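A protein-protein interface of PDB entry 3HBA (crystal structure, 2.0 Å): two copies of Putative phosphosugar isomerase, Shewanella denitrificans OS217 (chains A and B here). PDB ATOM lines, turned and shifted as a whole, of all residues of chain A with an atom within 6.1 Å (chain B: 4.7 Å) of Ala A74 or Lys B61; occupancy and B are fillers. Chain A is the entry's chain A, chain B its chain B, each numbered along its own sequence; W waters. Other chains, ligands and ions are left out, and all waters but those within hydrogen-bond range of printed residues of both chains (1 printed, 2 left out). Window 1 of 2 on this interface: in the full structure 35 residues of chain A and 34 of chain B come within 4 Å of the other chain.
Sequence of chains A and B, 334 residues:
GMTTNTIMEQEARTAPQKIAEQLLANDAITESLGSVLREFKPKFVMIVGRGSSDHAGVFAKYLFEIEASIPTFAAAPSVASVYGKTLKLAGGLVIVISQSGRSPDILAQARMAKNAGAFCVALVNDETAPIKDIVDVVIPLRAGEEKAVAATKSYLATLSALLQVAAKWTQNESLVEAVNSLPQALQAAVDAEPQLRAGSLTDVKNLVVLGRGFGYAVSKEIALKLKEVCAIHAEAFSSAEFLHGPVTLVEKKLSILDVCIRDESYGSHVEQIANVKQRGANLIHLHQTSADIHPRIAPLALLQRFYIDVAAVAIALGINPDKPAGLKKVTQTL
Water W1 bridges the backbone carbonyl oxygen of Ala A74 (2.8 Å) and the side-chain amino group of Lys B61 (3.1 Å).
2 positions are printed for both chains.
The side-chain amino group (NZ) of Lys B61 lies within salt-bridge range of the side-chain carboxylate (OE2) of Glu B65 (2.8 Å).
NZ of Lys B61 is in hydrogen-bond range of O of Thr B72 (2.8 Å).
The backbone NH of Thr B72 is in hydrogen-bond range of the side-chain carboxylate of Glu B65, at 3.0 Å.
O of Ala A74 is in hydrogen-bond range of NZ of Lys B61 (3.2 Å).
Of chain A, only Ala A74 and Ala A76 come within 4 Å of Lys B61.
Printed residues of chain B within 4 Å of Ala A76: Lys B61 and Tyr B62.
Of the printed residues of chain A, Tyr B62 touches Ala A76 and Val A79.
Of the printed residues of chain B, Val A79 touches Tyr B62 (3.9 Å) and Glu B65 (3.6 Å).
Printed residues of chain A within 4 Å of Glu B65: Val A79.
Of the 11 printed residues of chain B, 3 touch a printed residue of chain A.
Along chain B the printed residues that touch a printed residue of chain A span positions 61 to 65.
Hydrophobic or aromatic side chains of chain A within 4 Å of the printed part of chain B: Ala A76 and Val A79.
Among the printed residues, 5 pairs touch across the chains.
Ala A76 touches Lys B61.
Tyr B62 touches Ala A76 (OH to CB, 3.8 Å).
CG2 of Val A79 touches CD1 of Tyr B62, 3.9 Å away.
CG2 of Val A79 touches OE1 of Glu B65, at 3.6 Å.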
ATOM      1  N   VAL A  45     -12.556 -20.548  27.583  1.00  0.00           N
ATOM      2  CA  VAL A  45     -13.087 -21.911  27.541  1.00  0.00           C
ATOM      3  C   VAL A  45     -11.942 -22.877  27.255  1.00  0.00           C
ATOM      4  O   VAL A  45     -11.289 -22.788  26.229  1.00  0.00           O
ATOM      5  CB  VAL A  45     -14.197 -22.071  26.494  1.00  0.00           C
ATOM      6  CG1 VAL A  45     -14.723 -23.525  26.443  1.00  0.00           C
ATOM      7  CG2 VAL A  45     -15.366 -21.064  26.760  1.00  0.00           C
ATOM      8  N   MET A  46     -11.679 -23.781  28.192  1.00  0.00           N
ATOM      9  CA  MET A  46     -10.651 -24.780  27.990  1.00  0.00           C
ATOM     10  C   MET A  46     -11.280 -26.145  27.760  1.00  0.00           C
ATOM     11  O   MET A  46     -12.084 -26.640  28.596  1.00  0.00           O
ATOM     12  CB  MET A  46      -9.712 -24.831  29.184  1.00  0.00           C
ATOM     13  CG  MET A  46      -8.586 -25.808  29.007  1.00  0.00           C
ATOM     14  SD  MET A  46      -7.340 -25.702  30.529  1.00  0.00           S
ATOM     15  CE  MET A  46      -8.056 -27.098  31.613  1.00  0.00           C
ATOM     16  N   ILE A  47     -10.914 -26.771  26.642  1.00  0.00           N
ATOM     17  CA  ILE A  47     -11.454 -28.096  26.275  1.00  0.00           C
ATOM     18  C   ILE A  47     -10.514 -29.220  26.725  1.00  0.00           C
ATOM     19  O   ILE A  47      -9.346 -29.229  26.356  1.00  0.00           O
ATOM     20  CB  ILE A  47     -11.682 -28.215  24.756  1.00  0.00           C
ATOM     21  CG1 ILE A  47     -12.504 -27.013  24.226  1.00  0.00           C
ATOM     22  CG2 ILE A  47     -12.263 -29.603  24.450  1.00  0.00           C
ATOM     23  CD1 ILE A  47     -13.945 -26.887  24.789  1.00  0.00           C
ATOM     24  N   VAL A  48     -11.022 -30.142  27.547  1.00  0.00           N
ATOM     25  CA  VAL A  48     -10.249 -31.265  28.079  1.00  0.00           C
ATOM     26  C   VAL A  48     -10.670 -32.530  27.339  1.00  0.00           C
ATOM     27  O   VAL A  48     -11.851 -32.939  27.337  1.00  0.00           O
ATOM     28  CB  VAL A  48     -10.511 -31.455  29.586  1.00  0.00           C
ATOM     29  CG1 VAL A  48     -10.051 -32.821  30.051  1.00  0.00           C
ATOM     30  CG2 VAL A  48      -9.866 -30.340  30.378  1.00  0.00           C
ATOM     31  N   GLY A  51      -5.932 -33.779  24.046  1.00  0.00           N
ATOM     32  CA  GLY A  51      -4.929 -32.819  23.647  1.00  0.00           C
ATOM     33  C   GLY A  51      -5.265 -32.087  22.379  1.00  0.00           C
ATOM     34  O   GLY A  51      -6.432 -31.923  22.032  1.00  0.00           O
ATOM     35  N   SER A  52      -4.232 -31.621  21.683  1.00  0.00           N
ATOM     36  CA  SER A  52      -4.418 -30.905  20.410  1.00  0.00           C
ATOM     37  C   SER A  52      -4.964 -31.834  19.314  1.00  0.00           C
ATOM     38  O   SER A  52      -5.598 -31.378  18.352  1.00  0.00           O
ATOM     39  CB  SER A  52      -3.094 -30.270  19.965  1.00  0.00           C
ATOM     40  OG  SER A  52      -2.191 -31.251  19.498  1.00  0.00           O
ATOM     41  N   ASP A  54      -7.484 -33.362  19.490  1.00  0.00           N
ATOM     42  CA  ASP A  54      -8.876 -33.589  19.793  1.00  0.00           C
ATOM     43  C   ASP A  54      -9.711 -32.881  18.749  1.00  0.00           C
ATOM     44  O   ASP A  54      -9.792 -31.659  18.727  1.00  0.00           O
ATOM     45  CB  ASP A  54      -9.242 -33.155  21.193  1.00  0.00           C
ATOM     46  CG  ASP A  54     -10.511 -33.802  21.654  1.00  0.00           C
ATOM     47  OD1 ASP A  54     -11.598 -33.383  21.158  1.00  0.00           O
ATOM     48  OD2 ASP A  54     -10.404 -34.727  22.499  1.00  0.00           O
ATOM     49  N   GLY A  57     -12.506 -30.681  20.043  1.00  0.00           N
ATOM     50  CA  GLY A  57     -11.909 -29.489  20.630  1.00  0.00           C
ATOM     51  C   GLY A  57     -11.591 -28.431  19.570  1.00  0.00           C
ATOM     52  O   GLY A  57     -11.797 -27.260  19.791  1.00  0.00           O
ATOM     53  N   THR A  72     -10.974 -19.724  23.347  1.00  0.00           N
ATOM     54  CA  THR A  72     -11.202 -21.162  23.574  1.00  0.00           C
ATOM     55  C   THR A  72      -9.986 -21.958  23.116  1.00  0.00           C
ATOM     56  O   THR A  72      -9.365 -21.666  22.064  1.00  0.00           O
ATOM     57  CB  THR A  72     -12.461 -21.621  22.800  1.00  0.00           C
ATOM     58  OG1 THR A  72     -13.566 -20.808  23.228  1.00  0.00           O
ATOM     59  CG2 THR A  72     -12.768 -23.121  23.034  1.00  0.00           C
ATOM     60  N   PHE A  73      -9.591 -22.943  23.903  1.00  0.00           N
ATOM     61  CA  PHE A  73      -8.394 -23.699  23.558  1.00  0.00           C
ATOM     62  C   PHE A  73      -8.438 -25.095  24.151  1.00  0.00           C
ATOM     63  O   PHE A  73      -9.249 -25.386  25.016  1.00  0.00           O
ATOM     64  CB  PHE A  73      -7.139 -22.969  24.027  1.00  0.00           C
ATOM     65  CG  PHE A  73      -7.168 -22.617  25.467  1.00  0.00           C
ATOM     66  CD1 PHE A  73      -7.811 -21.455  25.888  1.00  0.00           C
ATOM     67  CD2 PHE A  73      -6.626 -23.462  26.413  1.00  0.00           C
ATOM     68  CE1 PHE A  73      -7.902 -21.167  27.220  1.00  0.00           C
ATOM     69  CE2 PHE A  73      -6.707 -23.163  27.751  1.00  0.00           C
ATOM     70  CZ  PHE A  73      -7.357 -22.019  28.155  1.00  0.00           C
ATOM     71  N   ALA A  74      -7.563 -25.946  23.654  1.00  0.00           N
ATOM     72  CA  ALA A  74      -7.431 -27.315  24.139  1.00  0.00           C
ATOM     73  C   ALA A  74      -6.388 -27.379  25.246  1.00  0.00           C
ATOM     74  O   ALA A  74      -5.298 -26.744  25.158  1.00  0.00           O
ATOM     75  CB  ALA A  74      -7.024 -28.262  22.981  1.00  0.00           C
ATOM     76  N   ALA A  75      -6.699 -28.154  26.279  1.00  0.00           N
ATOM     77  CA  ALA A  75      -5.712 -28.465  27.309  1.00  0.00           C
ATOM     78  C   ALA A  75      -4.703 -29.464  26.766  1.00  0.00           C
ATOM     79  O   ALA A  75      -5.027 -30.295  25.917  1.00  0.00           O
ATOM     80  CB  ALA A  75      -6.376 -29.091  28.585  1.00  0.00           C
ATOM     81  N   ALA A  76      -3.498 -29.423  27.335  1.00  0.00           N
ATOM     82  CA  ALA A  76      -2.447 -30.376  27.056  1.00  0.00           C
ATOM     83  C   ALA A  76      -2.459 -31.340  28.230  1.00  0.00           C
ATOM     84  O   ALA A  76      -2.091 -30.954  29.330  1.00  0.00           O
ATOM     85  CB  ALA A  76      -1.087 -29.643  26.969  1.00  0.00           C
ATOM     86  N   VAL A  79       0.399 -31.613  30.913  1.00  0.00           N
ATOM     87  CA  VAL A  79       0.606 -30.556  31.913  1.00  0.00           C
ATOM     88  C   VAL A  79       0.021 -30.977  33.265  1.00  0.00           C
ATOM     89  O   VAL A  79       0.721 -30.797  34.318  1.00  0.00           O
ATOM     90  CB  VAL A  79       0.098 -29.179  31.406  1.00  0.00           C
ATOM     91  CG1 VAL A  79       0.024 -28.154  32.514  1.00  0.00           C
ATOM     92  CG2 VAL A  79       1.035 -28.730  30.274  1.00  0.00           C
ATOM     93  N   GLY B  57       4.880 -21.293  19.616  1.00  0.00           N
ATOM     94  CA  GLY B  57       3.697 -21.224  20.469  1.00  0.00           C
ATOM     95  C   GLY B  57       3.384 -22.486  21.242  1.00  0.00           C
ATOM     96  O   GLY B  57       2.990 -22.410  22.391  1.00  0.00           O
ATOM     97  N   VAL B  58       3.581 -23.647  20.639  1.00  0.00           N
ATOM     98  CA  VAL B  58       3.443 -24.921  21.339  1.00  0.00           C
ATOM     99  C   VAL B  58       4.497 -25.013  22.457  1.00  0.00           C
ATOM    100  O   VAL B  58       4.207 -25.374  23.606  1.00  0.00           O
ATOM    101  CB  VAL B  58       3.576 -26.091  20.337  1.00  0.00           C
ATOM    102  CG1 VAL B  58       3.408 -27.425  21.017  1.00  0.00           C
ATOM    103  CG2 VAL B  58       2.553 -25.903  19.220  1.00  0.00           C
ATOM    104  N   PHE B  59       5.729 -24.622  22.159  1.00  0.00           N
ATOM    105  CA  PHE B  59       6.744 -24.562  23.218  1.00  0.00           C
ATOM    106  C   PHE B  59       6.298 -23.553  24.284  1.00  0.00           C
ATOM    107  O   PHE B  59       6.409 -23.815  25.476  1.00  0.00           O
ATOM    108  CB  PHE B  59       8.106 -24.156  22.651  1.00  0.00           C
ATOM    109  CG  PHE B  59       9.191 -24.132  23.671  1.00  0.00           C
ATOM    110  CD1 PHE B  59       9.927 -25.274  23.934  1.00  0.00           C
ATOM    111  CD2 PHE B  59       9.482 -22.960  24.372  1.00  0.00           C
ATOM    112  CE1 PHE B  59      10.899 -25.274  24.903  1.00  0.00           C
ATOM    113  CE2 PHE B  59      10.491 -22.948  25.351  1.00  0.00           C
ATOM    114  CZ  PHE B  59      11.188 -24.097  25.612  1.00  0.00           C
ATOM    115  N   ALA B  60       5.780 -22.394  23.850  1.00  0.00           N
ATOM    116  CA  ALA B  60       5.333 -21.375  24.824  1.00  0.00           C
ATOM    117  C   ALA B  60       4.242 -21.924  25.792  1.00  0.00           C
ATOM    118  O   ALA B  60       4.247 -21.614  26.987  1.00  0.00           O
ATOM    119  CB  ALA B  60       4.850 -20.106  24.108  1.00  0.00           C
ATOM    120  N   LYS B  61       3.337 -22.751  25.275  1.00  0.00           N
ATOM    121  CA  LYS B  61       2.267 -23.349  26.103  1.00  0.00           C
ATOM    122  C   LYS B  61       2.833 -24.158  27.250  1.00  0.00           C
ATOM    123  O   LYS B  61       2.499 -23.927  28.429  1.00  0.00           O
ATOM    124  CB  LYS B  61       1.302 -24.176  25.228  1.00  0.00           C
ATOM    125  CG  LYS B  61       0.200 -24.888  26.018  1.00  0.00           C
ATOM    126  CD  LYS B  61      -0.744 -25.698  25.114  1.00  0.00           C
ATOM    127  CE  LYS B  61      -1.922 -26.274  25.920  1.00  0.00           C
ATOM    128  NZ  LYS B  61      -2.824 -25.174  26.399  1.00  0.00           N
ATOM    129  N   TYR B  62       3.763 -25.055  26.941  1.00  0.00           N
ATOM    130  CA  TYR B  62       4.379 -25.856  27.992  1.00  0.00           C
ATOM    131  C   TYR B  62       5.106 -24.944  28.987  1.00  0.00           C
ATOM    132  O   TYR B  62       5.000 -25.122  30.198  1.00  0.00           O
ATOM    133  CB  TYR B  62       5.293 -26.923  27.373  1.00  0.00           C
ATOM    134  CG  TYR B  62       4.445 -27.987  26.744  1.00  0.00           C
ATOM    135  CD1 TYR B  62       3.855 -28.962  27.523  1.00  0.00           C
ATOM    136  CD2 TYR B  62       4.157 -27.965  25.389  1.00  0.00           C
ATOM    137  CE1 TYR B  62       3.037 -29.902  26.979  1.00  0.00           C
ATOM    138  CE2 TYR B  62       3.345 -28.902  24.837  1.00  0.00           C
ATOM    139  CZ  TYR B  62       2.773 -29.859  25.621  1.00  0.00           C
ATOM    140  OH  TYR B  62       1.958 -30.794  25.037  1.00  0.00           O
ATOM    141  N   LEU B  63       5.846 -23.975  28.463  1.00  0.00           N
ATOM    142  CA  LEU B  63       6.640 -23.084  29.306  1.00  0.00           C
ATOM    143  C   LEU B  63       5.806 -22.284  30.278  1.00  0.00           C
ATOM    144  O   LEU B  63       6.074 -22.303  31.480  1.00  0.00           O
ATOM    145  CB  LEU B  63       7.423 -22.100  28.417  1.00  0.00           C
ATOM    146  CG  LEU B  63       8.333 -21.066  29.094  1.00  0.00           C
ATOM    147  CD1 LEU B  63       9.461 -21.714  29.906  1.00  0.00           C
ATOM    148  CD2 LEU B  63       8.891 -20.168  27.926  1.00  0.00           C
ATOM    149  N   PHE B  64       4.828 -21.535  29.769  1.00  0.00           N
ATOM    150  CA  PHE B  64       4.056 -20.660  30.653  1.00  0.00           C
ATOM    151  C   PHE B  64       3.097 -21.429  31.524  1.00  0.00           C
ATOM    152  O   PHE B  64       2.889 -21.043  32.652  1.00  0.00           O
ATOM    153  CB  PHE B  64       3.381 -19.524  29.903  1.00  0.00           C
ATOM    154  CG  PHE B  64       4.371 -18.593  29.254  1.00  0.00           C
ATOM    155  CD1 PHE B  64       5.241 -17.843  30.024  1.00  0.00           C
ATOM    156  CD2 PHE B  64       4.422 -18.448  27.899  1.00  0.00           C
ATOM    157  CE1 PHE B  64       6.173 -17.004  29.436  1.00  0.00           C
ATOM    158  CE2 PHE B  64       5.367 -17.603  27.313  1.00  0.00           C
ATOM    159  CZ  PHE B  64       6.226 -16.883  28.076  1.00  0.00           C
ATOM    160  N   GLU B  65       2.562 -22.546  31.039  1.00  0.00           N
ATOM    161  CA  GLU B  65       1.620 -23.325  31.874  1.00  0.00           C
ATOM    162  C   GLU B  65       2.397 -24.026  32.985  1.00  0.00           C
ATOM    163  O   GLU B  65       1.962 -24.046  34.144  1.00  0.00           O
ATOM    164  CB  GLU B  65       0.827 -24.349  31.061  1.00  0.00           C
ATOM    165  CG  GLU B  65      -0.172 -23.739  30.132  1.00  0.00           C
ATOM    166  CD  GLU B  65      -1.217 -24.687  29.593  1.00  0.00           C
ATOM    167  OE1 GLU B  65      -1.147 -25.951  29.733  1.00  0.00           O
ATOM    168  OE2 GLU B  65      -2.123 -24.127  28.954  1.00  0.00           O
ATOM    169  N   ILE B  66       3.580 -24.545  32.664  1.00  0.00           N
ATOM    170  CA  ILE B  66       4.356 -25.269  33.705  1.00  0.00           C
ATOM    171  C   ILE B  66       5.078 -24.341  34.671  1.00  0.00           C
ATOM    172  O   ILE B  66       5.061 -24.564  35.888  1.00  0.00           O
ATOM    173  CB  ILE B  66       5.299 -26.287  33.081  1.00  0.00           C
ATOM    174  CG1 ILE B  66       4.462 -27.392  32.431  1.00  0.00           C
ATOM    175  CG2 ILE B  66       6.270 -26.862  34.130  1.00  0.00           C
ATOM    176  CD1 ILE B  66       5.193 -28.228  31.428  1.00  0.00           C
ATOM    177  N   THR B  72      -2.215 -21.185  28.427  1.00  0.00           N
ATOM    178  CA  THR B  72      -1.570 -20.574  27.282  1.00  0.00           C
ATOM    179  C   THR B  72      -2.020 -21.281  26.026  1.00  0.00           C
ATOM    180  O   THR B  72      -2.150 -22.509  26.013  1.00  0.00           O
ATOM    181  CB  THR B  72       0.001 -20.687  27.424  1.00  0.00           C
ATOM    182  OG1 THR B  72       0.443 -20.027  28.613  1.00  0.00           O
ATOM    183  CG2 THR B  72       0.732 -20.134  26.255  1.00  0.00           C
HETATM  184  O   HOH W   1      -3.914 -24.985  23.506  1.00  0.00           O
